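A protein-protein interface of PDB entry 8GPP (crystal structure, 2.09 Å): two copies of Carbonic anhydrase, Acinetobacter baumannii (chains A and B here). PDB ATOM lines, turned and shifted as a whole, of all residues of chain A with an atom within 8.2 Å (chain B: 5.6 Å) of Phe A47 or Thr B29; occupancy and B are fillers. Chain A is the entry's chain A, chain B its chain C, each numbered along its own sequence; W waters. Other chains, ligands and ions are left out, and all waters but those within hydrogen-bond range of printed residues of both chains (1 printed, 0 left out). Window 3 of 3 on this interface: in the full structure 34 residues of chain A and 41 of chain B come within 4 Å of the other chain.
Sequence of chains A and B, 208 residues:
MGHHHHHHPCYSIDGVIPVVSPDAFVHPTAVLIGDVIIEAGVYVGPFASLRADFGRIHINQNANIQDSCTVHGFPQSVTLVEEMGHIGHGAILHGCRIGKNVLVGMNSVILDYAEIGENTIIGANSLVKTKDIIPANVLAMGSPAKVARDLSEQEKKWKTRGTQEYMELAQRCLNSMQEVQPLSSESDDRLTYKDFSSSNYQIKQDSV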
ATOM      1  N   HIS A  27     -21.866  -8.188  -2.593  1.00  0.00           N
ATOM      2  CA  HIS A  27     -22.280  -9.581  -2.703  1.00  0.00           C
ATOM      3  C   HIS A  27     -23.801  -9.671  -2.807  1.00  0.00           C
ATOM      4  O   HIS A  27     -24.517  -8.860  -2.210  1.00  0.00           O
ATOM      5  CB  HIS A  27     -21.803 -10.417  -1.526  1.00  0.00           C
ATOM      6  CG  HIS A  27     -21.877 -11.889  -1.793  1.00  0.00           C
ATOM      7  ND1 HIS A  27     -22.981 -12.652  -1.472  1.00  0.00           N
ATOM      8  CD2 HIS A  27     -20.992 -12.734  -2.376  1.00  0.00           C
ATOM      9  CE1 HIS A  27     -22.774 -13.901  -1.845  1.00  0.00           C
ATOM     10  NE2 HIS A  27     -21.576 -13.978  -2.394  1.00  0.00           N
ATOM     11  N   PRO A  28     -24.326 -10.605  -3.602  1.00  0.00           N
ATOM     12  CA  PRO A  28     -25.785 -10.665  -3.804  1.00  0.00           C
ATOM     13  C   PRO A  28     -26.580 -10.976  -2.547  1.00  0.00           C
ATOM     14  O   PRO A  28     -27.800 -10.790  -2.553  1.00  0.00           O
ATOM     15  CB  PRO A  28     -25.960 -11.771  -4.857  1.00  0.00           C
ATOM     16  CG  PRO A  28     -24.604 -11.994  -5.484  1.00  0.00           C
ATOM     17  CD  PRO A  28     -23.558 -11.403  -4.585  1.00  0.00           C
ATOM     18  N   THR A  29     -25.944 -11.458  -1.481  1.00  0.00           N
ATOM     19  CA  THR A  29     -26.631 -11.730  -0.232  1.00  0.00           C
ATOM     20  C   THR A  29     -26.452 -10.622   0.790  1.00  0.00           C
ATOM     21  O   THR A  29     -26.835 -10.802   1.950  1.00  0.00           O
ATOM     22  CB  THR A  29     -26.139 -13.043   0.379  1.00  0.00           C
ATOM     23  OG1 THR A  29     -24.775 -12.879   0.764  1.00  0.00           O
ATOM     24  CG2 THR A  29     -26.264 -14.196  -0.611  1.00  0.00           C
ATOM     25  N   ALA A  30     -25.825  -9.517   0.412  1.00  0.00           N
ATOM     26  CA  ALA A  30     -25.851  -8.341   1.252  1.00  0.00           C
ATOM     27  C   ALA A  30     -27.217  -7.675   1.140  1.00  0.00           C
ATOM     28  O   ALA A  30     -28.032  -8.022   0.292  1.00  0.00           O
ATOM     29  CB  ALA A  30     -24.740  -7.364   0.845  1.00  0.00           C
ATOM     30  N   VAL A  31     -27.482  -6.725   2.022  1.00  0.00           N
ATOM     31  CA  VAL A  31     -28.719  -5.953   1.955  1.00  0.00           C
ATOM     32  C   VAL A  31     -28.370  -4.481   2.122  1.00  0.00           C
ATOM     33  O   VAL A  31     -27.731  -4.101   3.112  1.00  0.00           O
ATOM     34  CB  VAL A  31     -29.747  -6.408   3.009  1.00  0.00           C
ATOM     35  CG1 VAL A  31     -30.797  -5.317   3.268  1.00  0.00           C
ATOM     36  CG2 VAL A  31     -30.429  -7.696   2.549  1.00  0.00           C
ATOM     37  N   VAL A  44     -18.424  -5.200  -0.432  1.00  0.00           N
ATOM     38  CA  VAL A  44     -19.427  -5.524   0.583  1.00  0.00           C
ATOM     39  C   VAL A  44     -19.677  -7.028   0.543  1.00  0.00           C
ATOM     40  O   VAL A  44     -20.160  -7.555  -0.473  1.00  0.00           O
ATOM     41  CB  VAL A  44     -20.739  -4.752   0.376  1.00  0.00           C
ATOM     42  CG1 VAL A  44     -21.683  -4.968   1.584  1.00  0.00           C
ATOM     43  CG2 VAL A  44     -20.454  -3.271   0.164  1.00  0.00           C
ATOM     44  N   GLY A  45     -19.390  -7.707   1.659  1.00  0.00           N
ATOM     45  CA  GLY A  45     -19.440  -9.153   1.718  1.00  0.00           C
ATOM     46  C   GLY A  45     -20.789  -9.732   2.115  1.00  0.00           C
ATOM     47  O   GLY A  45     -21.765  -9.006   2.359  1.00  0.00           O
ATOM     48  N   PRO A  46     -20.859 -11.068   2.194  1.00  0.00           N
ATOM     49  CA  PRO A  46     -22.146 -11.734   2.458  1.00  0.00           C
ATOM     50  C   PRO A  46     -22.775 -11.281   3.763  1.00  0.00           C
ATOM     51  O   PRO A  46     -22.098 -11.125   4.785  1.00  0.00           O
ATOM     52  CB  PRO A  46     -21.784 -13.229   2.504  1.00  0.00           C
ATOM     53  CG  PRO A  46     -20.476 -13.344   1.736  1.00  0.00           C
ATOM     54  CD  PRO A  46     -19.806 -11.996   1.740  1.00  0.00           C
ATOM     55  N   PHE A  47     -24.088 -11.049   3.711  1.00  0.00           N
ATOM     56  CA  PHE A  47     -24.906 -10.748   4.888  1.00  0.00           C
ATOM     57  C   PHE A  47     -24.527  -9.438   5.562  1.00  0.00           C
ATOM     58  O   PHE A  47     -24.896  -9.202   6.718  1.00  0.00           O
ATOM     59  CB  PHE A  47     -24.845 -11.888   5.910  1.00  0.00           C
ATOM     60  CG  PHE A  47     -24.937 -13.220   5.292  1.00  0.00           C
ATOM     61  CD1 PHE A  47     -25.978 -13.517   4.441  1.00  0.00           C
ATOM     62  CD2 PHE A  47     -23.969 -14.169   5.520  1.00  0.00           C
ATOM     63  CE1 PHE A  47     -26.052 -14.746   3.826  1.00  0.00           C
ATOM     64  CE2 PHE A  47     -24.051 -15.400   4.924  1.00  0.00           C
ATOM     65  CZ  PHE A  47     -25.100 -15.690   4.076  1.00  0.00           C
ATOM     66  N   ALA A  48     -23.825  -8.562   4.858  1.00  0.00           N
ATOM     67  CA  ALA A  48     -23.638  -7.220   5.367  1.00  0.00           C
ATOM     68  C   ALA A  48     -24.947  -6.455   5.226  1.00  0.00           C
ATOM     69  O   ALA A  48     -25.555  -6.439   4.152  1.00  0.00           O
ATOM     70  CB  ALA A  48     -22.513  -6.512   4.620  1.00  0.00           C
ATOM     71  N   SER A  49     -25.405  -5.849   6.315  1.00  0.00           N
ATOM     72  CA  SER A  49     -26.627  -5.043   6.284  1.00  0.00           C
ATOM     73  C   SER A  49     -26.240  -3.572   6.380  1.00  0.00           C
ATOM     74  O   SER A  49     -25.745  -3.113   7.414  1.00  0.00           O
ATOM     75  CB  SER A  49     -27.586  -5.427   7.398  1.00  0.00           C
ATOM     76  OG  SER A  49     -28.775  -4.649   7.323  1.00  0.00           O
ATOM     77  N   LEU A  50     -26.419  -2.849   5.292  1.00  0.00           N
ATOM     78  CA  LEU A  50     -26.230  -1.405   5.281  1.00  0.00           C
ATOM     79  C   LEU A  50     -27.646  -0.870   5.314  1.00  0.00           C
ATOM     80  O   LEU A  50     -28.322  -0.775   4.291  1.00  0.00           O
ATOM     81  CB  LEU A  50     -25.436  -0.932   4.060  1.00  0.00           C
ATOM     82  CG  LEU A  50     -23.925  -1.237   4.114  1.00  0.00           C
ATOM     83  CD1 LEU A  50     -23.664  -2.585   4.726  1.00  0.00           C
ATOM     84  CD2 LEU A  50     -23.253  -1.161   2.739  1.00  0.00           C
ATOM     85  N   ILE A  65     -16.643  -3.785   3.677  1.00  0.00           N
ATOM     86  CA  ILE A  65     -17.571  -4.199   4.713  1.00  0.00           C
ATOM     87  C   ILE A  65     -17.669  -5.717   4.618  1.00  0.00           C
ATOM     88  O   ILE A  65     -18.096  -6.251   3.587  1.00  0.00           O
ATOM     89  CB  ILE A  65     -18.949  -3.550   4.520  1.00  0.00           C
ATOM     90  CG1 ILE A  65     -18.807  -2.085   4.093  1.00  0.00           C
ATOM     91  CG2 ILE A  65     -19.809  -3.696   5.790  1.00  0.00           C
ATOM     92  CD1 ILE A  65     -18.597  -1.126   5.232  1.00  0.00           C
ATOM     93  N   GLN A  66     -17.303  -6.411   5.691  1.00  0.00           N
ATOM     94  CA  GLN A  66     -17.152  -7.856   5.632  1.00  0.00           C
ATOM     95  C   GLN A  66     -18.436  -8.556   6.080  1.00  0.00           C
ATOM     96  O   GLN A  66     -19.481  -7.928   6.280  1.00  0.00           O
ATOM     97  CB  GLN A  66     -15.932  -8.270   6.453  1.00  0.00           C
ATOM     98  CG  GLN A  66     -14.643  -7.880   5.752  1.00  0.00           C
ATOM     99  CD  GLN A  66     -13.410  -7.980   6.605  1.00  0.00           C
ATOM    100  OE1 GLN A  66     -13.347  -8.773   7.543  1.00  0.00           O
ATOM    101  NE2 GLN A  66     -12.402  -7.171   6.278  1.00  0.00           N
ATOM    102  N   ASP A  67     -18.359  -9.884   6.215  1.00  0.00           N
ATOM    103  CA  ASP A  67     -19.527 -10.740   6.349  1.00  0.00           C
ATOM    104  C   ASP A  67     -20.292 -10.454   7.638  1.00  0.00           C
ATOM    105  O   ASP A  67     -19.705 -10.295   8.714  1.00  0.00           O
ATOM    106  CB  ASP A  67     -19.099 -12.220   6.306  1.00  0.00           C
ATOM    107  CG  ASP A  67     -17.840 -12.438   5.462  1.00  0.00           C
ATOM    108  OD1 ASP A  67     -16.767 -11.908   5.838  1.00  0.00           O
ATOM    109  OD2 ASP A  67     -17.925 -13.142   4.426  1.00  0.00           O
ATOM    110  N   SER A  68     -21.615 -10.405   7.518  1.00  0.00           N
ATOM    111  CA  SER A  68     -22.513 -10.181   8.652  1.00  0.00           C
ATOM    112  C   SER A  68     -22.164  -8.906   9.409  1.00  0.00           C
ATOM    113  O   SER A  68     -22.466  -8.788  10.582  1.00  0.00           O
ATOM    114  CB  SER A  68     -22.501 -11.371   9.620  1.00  0.00           C
ATOM    115  OG  SER A  68     -23.020 -12.534   9.004  1.00  0.00           O
ATOM    116  N   CYS A  69     -21.503  -7.957   8.767  1.00  0.00           N
ATOM    117  CA  CYS A  69     -21.388  -6.639   9.343  1.00  0.00           C
ATOM    118  C   CYS A  69     -22.740  -5.938   9.286  1.00  0.00           C
ATOM    119  O   CYS A  69     -23.604  -6.263   8.462  1.00  0.00           O
ATOM    120  CB  CYS A  69     -20.329  -5.827   8.603  1.00  0.00           C
ATOM    121  SG  CYS A  69     -18.629  -6.404   8.898  1.00  0.00           S
ATOM    122  N   THR A  70     -22.930  -4.977  10.186  1.00  0.00           N
ATOM    123  CA  THR A  70     -24.136  -4.163  10.171  1.00  0.00           C
ATOM    124  C   THR A  70     -23.771  -2.692  10.299  1.00  0.00           C
ATOM    125  O   THR A  70     -23.009  -2.300  11.192  1.00  0.00           O
ATOM    126  CB  THR A  70     -25.098  -4.607  11.279  1.00  0.00           C
ATOM    127  OG1 THR A  70     -25.489  -5.961  11.012  1.00  0.00           O
ATOM    128  CG2 THR A  70     -26.354  -3.714  11.338  1.00  0.00           C
ATOM    129  N   VAL A  71     -24.325  -1.881   9.409  1.00  0.00           N
ATOM    130  CA  VAL A  71     -24.177  -0.435   9.465  1.00  0.00           C
ATOM    131  C   VAL A  71     -25.566   0.159   9.618  1.00  0.00           C
ATOM    132  O   VAL A  71     -26.425  -0.033   8.748  1.00  0.00           O
ATOM    133  CB  VAL A  71     -23.477   0.134   8.219  1.00  0.00           C
ATOM    134  CG1 VAL A  71     -23.147   1.597   8.466  1.00  0.00           C
ATOM    135  CG2 VAL A  71     -22.205  -0.649   7.904  1.00  0.00           C
ATOM    136  N   GLY A  90     -18.408  -9.283  11.138  1.00  0.00           N
ATOM    137  CA  GLY A  90     -19.291  -9.191  12.278  1.00  0.00           C
ATOM    138  C   GLY A  90     -19.300  -7.871  13.026  1.00  0.00           C
ATOM    139  O   GLY A  90     -20.087  -7.731  13.976  1.00  0.00           O
ATOM    140  N   ALA A  91     -18.461  -6.910  12.647  1.00  0.00           N
ATOM    141  CA  ALA A  91     -18.436  -5.618  13.319  1.00  0.00           C
ATOM    142  C   ALA A  91     -19.713  -4.844  13.026  1.00  0.00           C
ATOM    143  O   ALA A  91     -20.313  -4.981  11.958  1.00  0.00           O
ATOM    144  CB  ALA A  91     -17.211  -4.799  12.881  1.00  0.00           C
ATOM    145  N   PRO B   9     -26.582 -22.625  -2.285  1.00  0.00           N
ATOM    146  CA  PRO B   9     -26.025 -21.287  -2.460  1.00  0.00           C
ATOM    147  C   PRO B   9     -24.512 -21.232  -2.538  1.00  0.00           C
ATOM    148  O   PRO B   9     -23.871 -20.803  -1.615  1.00  0.00           O
ATOM    149  CB  PRO B   9     -26.469 -20.604  -1.201  1.00  0.00           C
ATOM    150  CG  PRO B   9     -26.374 -21.683  -0.202  1.00  0.00           C
ATOM    151  CD  PRO B   9     -26.841 -22.920  -0.879  1.00  0.00           C
ATOM    152  N   HIS B  27     -28.000 -24.792   4.703  1.00  0.00           N
ATOM    153  CA  HIS B  27     -29.234 -24.036   4.575  1.00  0.00           C
ATOM    154  C   HIS B  27     -29.170 -23.172   3.315  1.00  0.00           C
ATOM    155  O   HIS B  27     -28.099 -22.658   2.965  1.00  0.00           O
ATOM    156  CB  HIS B  27     -29.475 -23.158   5.796  1.00  0.00           C
ATOM    157  CG  HIS B  27     -30.882 -22.670   5.887  1.00  0.00           C
ATOM    158  ND1 HIS B  27     -31.305 -21.514   5.270  1.00  0.00           N
ATOM    159  CD2 HIS B  27     -31.972 -23.200   6.489  1.00  0.00           C
ATOM    160  CE1 HIS B  27     -32.597 -21.349   5.497  1.00  0.00           C
ATOM    161  NE2 HIS B  27     -33.028 -22.366   6.225  1.00  0.00           N
ATOM    162  N   PRO B  28     -30.281 -23.009   2.598  1.00  0.00           N
ATOM    163  CA  PRO B  28     -30.220 -22.250   1.341  1.00  0.00           C
ATOM    164  C   PRO B  28     -29.763 -20.811   1.510  1.00  0.00           C
ATOM    165  O   PRO B  28     -29.392 -20.187   0.507  1.00  0.00           O
ATOM    166  CB  PRO B  28     -31.655 -22.328   0.792  1.00  0.00           C
ATOM    167  CG  PRO B  28     -32.339 -23.421   1.545  1.00  0.00           C
ATOM    168  CD  PRO B  28     -31.472 -23.872   2.691  1.00  0.00           C
ATOM    169  N   THR B  29     -29.765 -20.258   2.728  1.00  0.00           N
ATOM    170  CA  THR B  29     -29.316 -18.883   2.932  1.00  0.00           C
ATOM    171  C   THR B  29     -27.906 -18.788   3.479  1.00  0.00           C
ATOM    172  O   THR B  29     -27.484 -17.689   3.870  1.00  0.00           O
ATOM    173  CB  THR B  29     -30.231 -18.132   3.898  1.00  0.00           C
ATOM    174  OG1 THR B  29     -30.066 -18.702   5.201  1.00  0.00           O
ATOM    175  CG2 THR B  29     -31.700 -18.181   3.445  1.00  0.00           C
ATOM    176  N   ALA B  30     -27.208 -19.911   3.615  1.00  0.00           N
ATOM    177  CA  ALA B  30     -25.777 -19.861   3.806  1.00  0.00           C
ATOM    178  C   ALA B  30     -25.129 -19.387   2.516  1.00  0.00           C
ATOM    179  O   ALA B  30     -25.752 -19.366   1.452  1.00  0.00           O
ATOM    180  CB  ALA B  30     -25.215 -21.240   4.182  1.00  0.00           C
ATOM    181  N   VAL B  31     -23.854 -19.024   2.617  1.00  0.00           N
ATOM    182  CA  VAL B  31     -23.044 -18.679   1.458  1.00  0.00           C
ATOM    183  C   VAL B  31     -21.752 -19.463   1.542  1.00  0.00           C
ATOM    184  O   VAL B  31     -21.041 -19.395   2.554  1.00  0.00           O
ATOM    185  CB  VAL B  31     -22.741 -17.172   1.381  1.00  0.00           C
ATOM    186  CG1 VAL B  31     -21.486 -16.904   0.502  1.00  0.00           C
ATOM    187  CG2 VAL B  31     -23.965 -16.417   0.861  1.00  0.00           C
ATOM    188  N   GLY B  45     -25.840 -23.534   9.013  1.00  0.00           N
ATOM    189  CA  GLY B  45     -27.057 -22.838   9.323  1.00  0.00           C
ATOM    190  C   GLY B  45     -27.240 -21.542   8.554  1.00  0.00           C
ATOM    191  O   GLY B  45     -26.407 -21.131   7.736  1.00  0.00           O
ATOM    192  N   PRO B  46     -28.370 -20.889   8.808  1.00  0.00           N
ATOM    193  CA  PRO B  46     -28.695 -19.648   8.101  1.00  0.00           C
ATOM    194  C   PRO B  46     -27.608 -18.591   8.233  1.00  0.00           C
ATOM    195  O   PRO B  46     -27.092 -18.327   9.323  1.00  0.00           O
ATOM    196  CB  PRO B  46     -29.995 -19.189   8.766  1.00  0.00           C
ATOM    197  CG  PRO B  46     -30.534 -20.391   9.490  1.00  0.00           C
ATOM    198  CD  PRO B  46     -29.525 -21.471   9.515  1.00  0.00           C
ATOM    199  N   PHE B  47     -27.281 -17.978   7.096  1.00  0.00           N
ATOM    200  CA  PHE B  47     -26.353 -16.850   6.998  1.00  0.00           C
ATOM    201  C   PHE B  47     -24.949 -17.187   7.479  1.00  0.00           C
ATOM    202  O   PHE B  47     -24.202 -16.291   7.868  1.00  0.00           O
ATOM    203  CB  PHE B  47     -26.873 -15.627   7.762  1.00  0.00           C
ATOM    204  CG  PHE B  47     -28.353 -15.454   7.684  1.00  0.00           C
ATOM    205  CD1 PHE B  47     -28.971 -15.196   6.471  1.00  0.00           C
ATOM    206  CD2 PHE B  47     -29.132 -15.544   8.827  1.00  0.00           C
ATOM    207  CE1 PHE B  47     -30.352 -15.046   6.405  1.00  0.00           C
ATOM    208  CE2 PHE B  47     -30.500 -15.385   8.763  1.00  0.00           C
ATOM    209  CZ  PHE B  47     -31.112 -15.133   7.555  1.00  0.00           C
ATOM    210  N   ALA B  48     -24.579 -18.462   7.506  1.00  0.00           N
ATOM    211  CA  ALA B  48     -23.182 -18.789   7.706  1.00  0.00           C
ATOM    212  C   ALA B  48     -22.429 -18.446   6.430  1.00  0.00           C
ATOM    213  O   ALA B  48     -22.854 -18.816   5.327  1.00  0.00           O
ATOM    214  CB  ALA B  48     -22.998 -20.263   8.051  1.00  0.00           C
ATOM    215  N   SER B  49     -21.341 -17.697   6.566  1.00  0.00           N
ATOM    216  CA  SER B  49     -20.499 -17.361   5.424  1.00  0.00           C
ATOM    217  C   SER B  49     -19.220 -18.175   5.529  1.00  0.00           C
ATOM    218  O   SER B  49     -18.394 -17.935   6.411  1.00  0.00           O
ATOM    219  CB  SER B  49     -20.200 -15.871   5.376  1.00  0.00           C
ATOM    220  OG  SER B  49     -19.415 -15.587   4.235  1.00  0.00           O
HETATM  221  O   HOH W   1     -21.745 -14.662   8.368  1.00  0.00           O
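The side-chain carboxylate of Asp A67 is in hydrogen-bond range of the side-chain hydroxyl of Ser B49, at 2.9 Å.
A ring nitrogen (ND1) of His A27 is in hydrogen-bond range of the side-chain hydroxyl (OG1) of Thr A29, at 2.9 Å.
The backbone carbonyl oxygen of Val A44 sits at hydrogen-bond distance from the backbone NH of His A27 (2.8 Å).
The backbone carbonyl oxygen (O) of Pro A46 sits at hydrogen-bond distance from the backbone NH (N) of Ser A68.
O of Asp A67 sits at hydrogen-bond distance from N of Gly A90.
A ring nitrogen (ND1) of His B27 lies within hydrogen-bond range of the side-chain hydroxyl (OG1) of Thr B29 (3.1 Å).
The backbone NH (N) of Val B31 sits at hydrogen-bond distance from the backbone carbonyl oxygen (O) of Ala B48 (2.9 Å).
CG2 of Val B31 touches CE1 of His A27, at 3.9 Å.
CG2 of Thr A29 touches CG2 of Val B31, at 3.5 Å.
Val B31 touches Pro A46 (CG1 to CG, 3.9 Å).
OG of Ser B49 touches CG of Pro A46, 3.5 Å away.
CZ of Phe A47 touches O of Thr B29 (3.1 Å).
Val B31 touches Phe A47 (CG2 to CZ, 3.5 Å).
Phe A47 touches Phe B47.
Ala B48 touches Phe A47 (O to CE2, 3.6 Å).
Phe A47 touches Ser B49.
Of the printed residues of chain B, His A27 touches Val B31 (3.9 Å).
Printed residues of chain B within 4 Å of Thr A29: Val B31 (3.5 Å).
Printed residues of chain B within 4 Å of Phe A47: Thr B29 (3.1 Å), Val B31 (3.5 Å), Phe B47 (3.1 Å), Ala B48 (3.6 Å) and Ser B49 (3.9 Å).
Thr B29 touches one residue of chain A.
The nearest residue of chain A that does not touch Thr B29 is Thr A29 (5.8 Å).
The nearest printed residue of chain B that does not touch Asp A67 is Val B31 (6.5 Å).
Printed residues of chain A that touch a printed residue of chain B: His A27, Thr A29, Pro A46, Phe A47 and Asp A67.
Hydrophobic or aromatic side chains of chain A that line the printed part of chain B: His A27, Pro A46 and Phe A47.
Printed residues of chain B that touch a printed residue of chain A: Thr B29, Val B31, Phe B47, Ala B48 and Ser B49.
Hydrophobic or aromatic side chains of chain B within 4 Å of the printed part of chain A: Val B31 and Phe B47.
Among the printed residues, 10 pairs touch across the chains.
Among the printed residues, no Asp or Glu carboxylate lies within 4 Å of a Lys or Arg side-chain nitrogen of the other chain.
Thr A29 touches Val B31, but with the chains exchanged Val A31 does not touch Thr B29 (10.5 Å).
Pro A46 touches Val B31, but with the chains exchanged Val A31 does not touch Pro B46 (12.6 Å).
Phe A47 touches Ala B48, but with the chains exchanged Ala A48 does not touch Phe B47 (8.2 Å).
Phe A47 touches Ser B49, but with the chains exchanged Ser A49 does not touch Phe B47 (9.9 Å).
Positions printed for both chains: 27, 28, 29, 30, 31, 45, 46, 47, 48 and 49.
Of the 10 pairs that touch across the chains among the printed residues, 1 has its exchanged pair printed and touching as well.
Water W1 bridges the side-chain hydroxyl (OG) of Ser A68 (2.6 Å) and the backbone carbonyl oxygen (O) of Phe B47 (3.0 Å).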
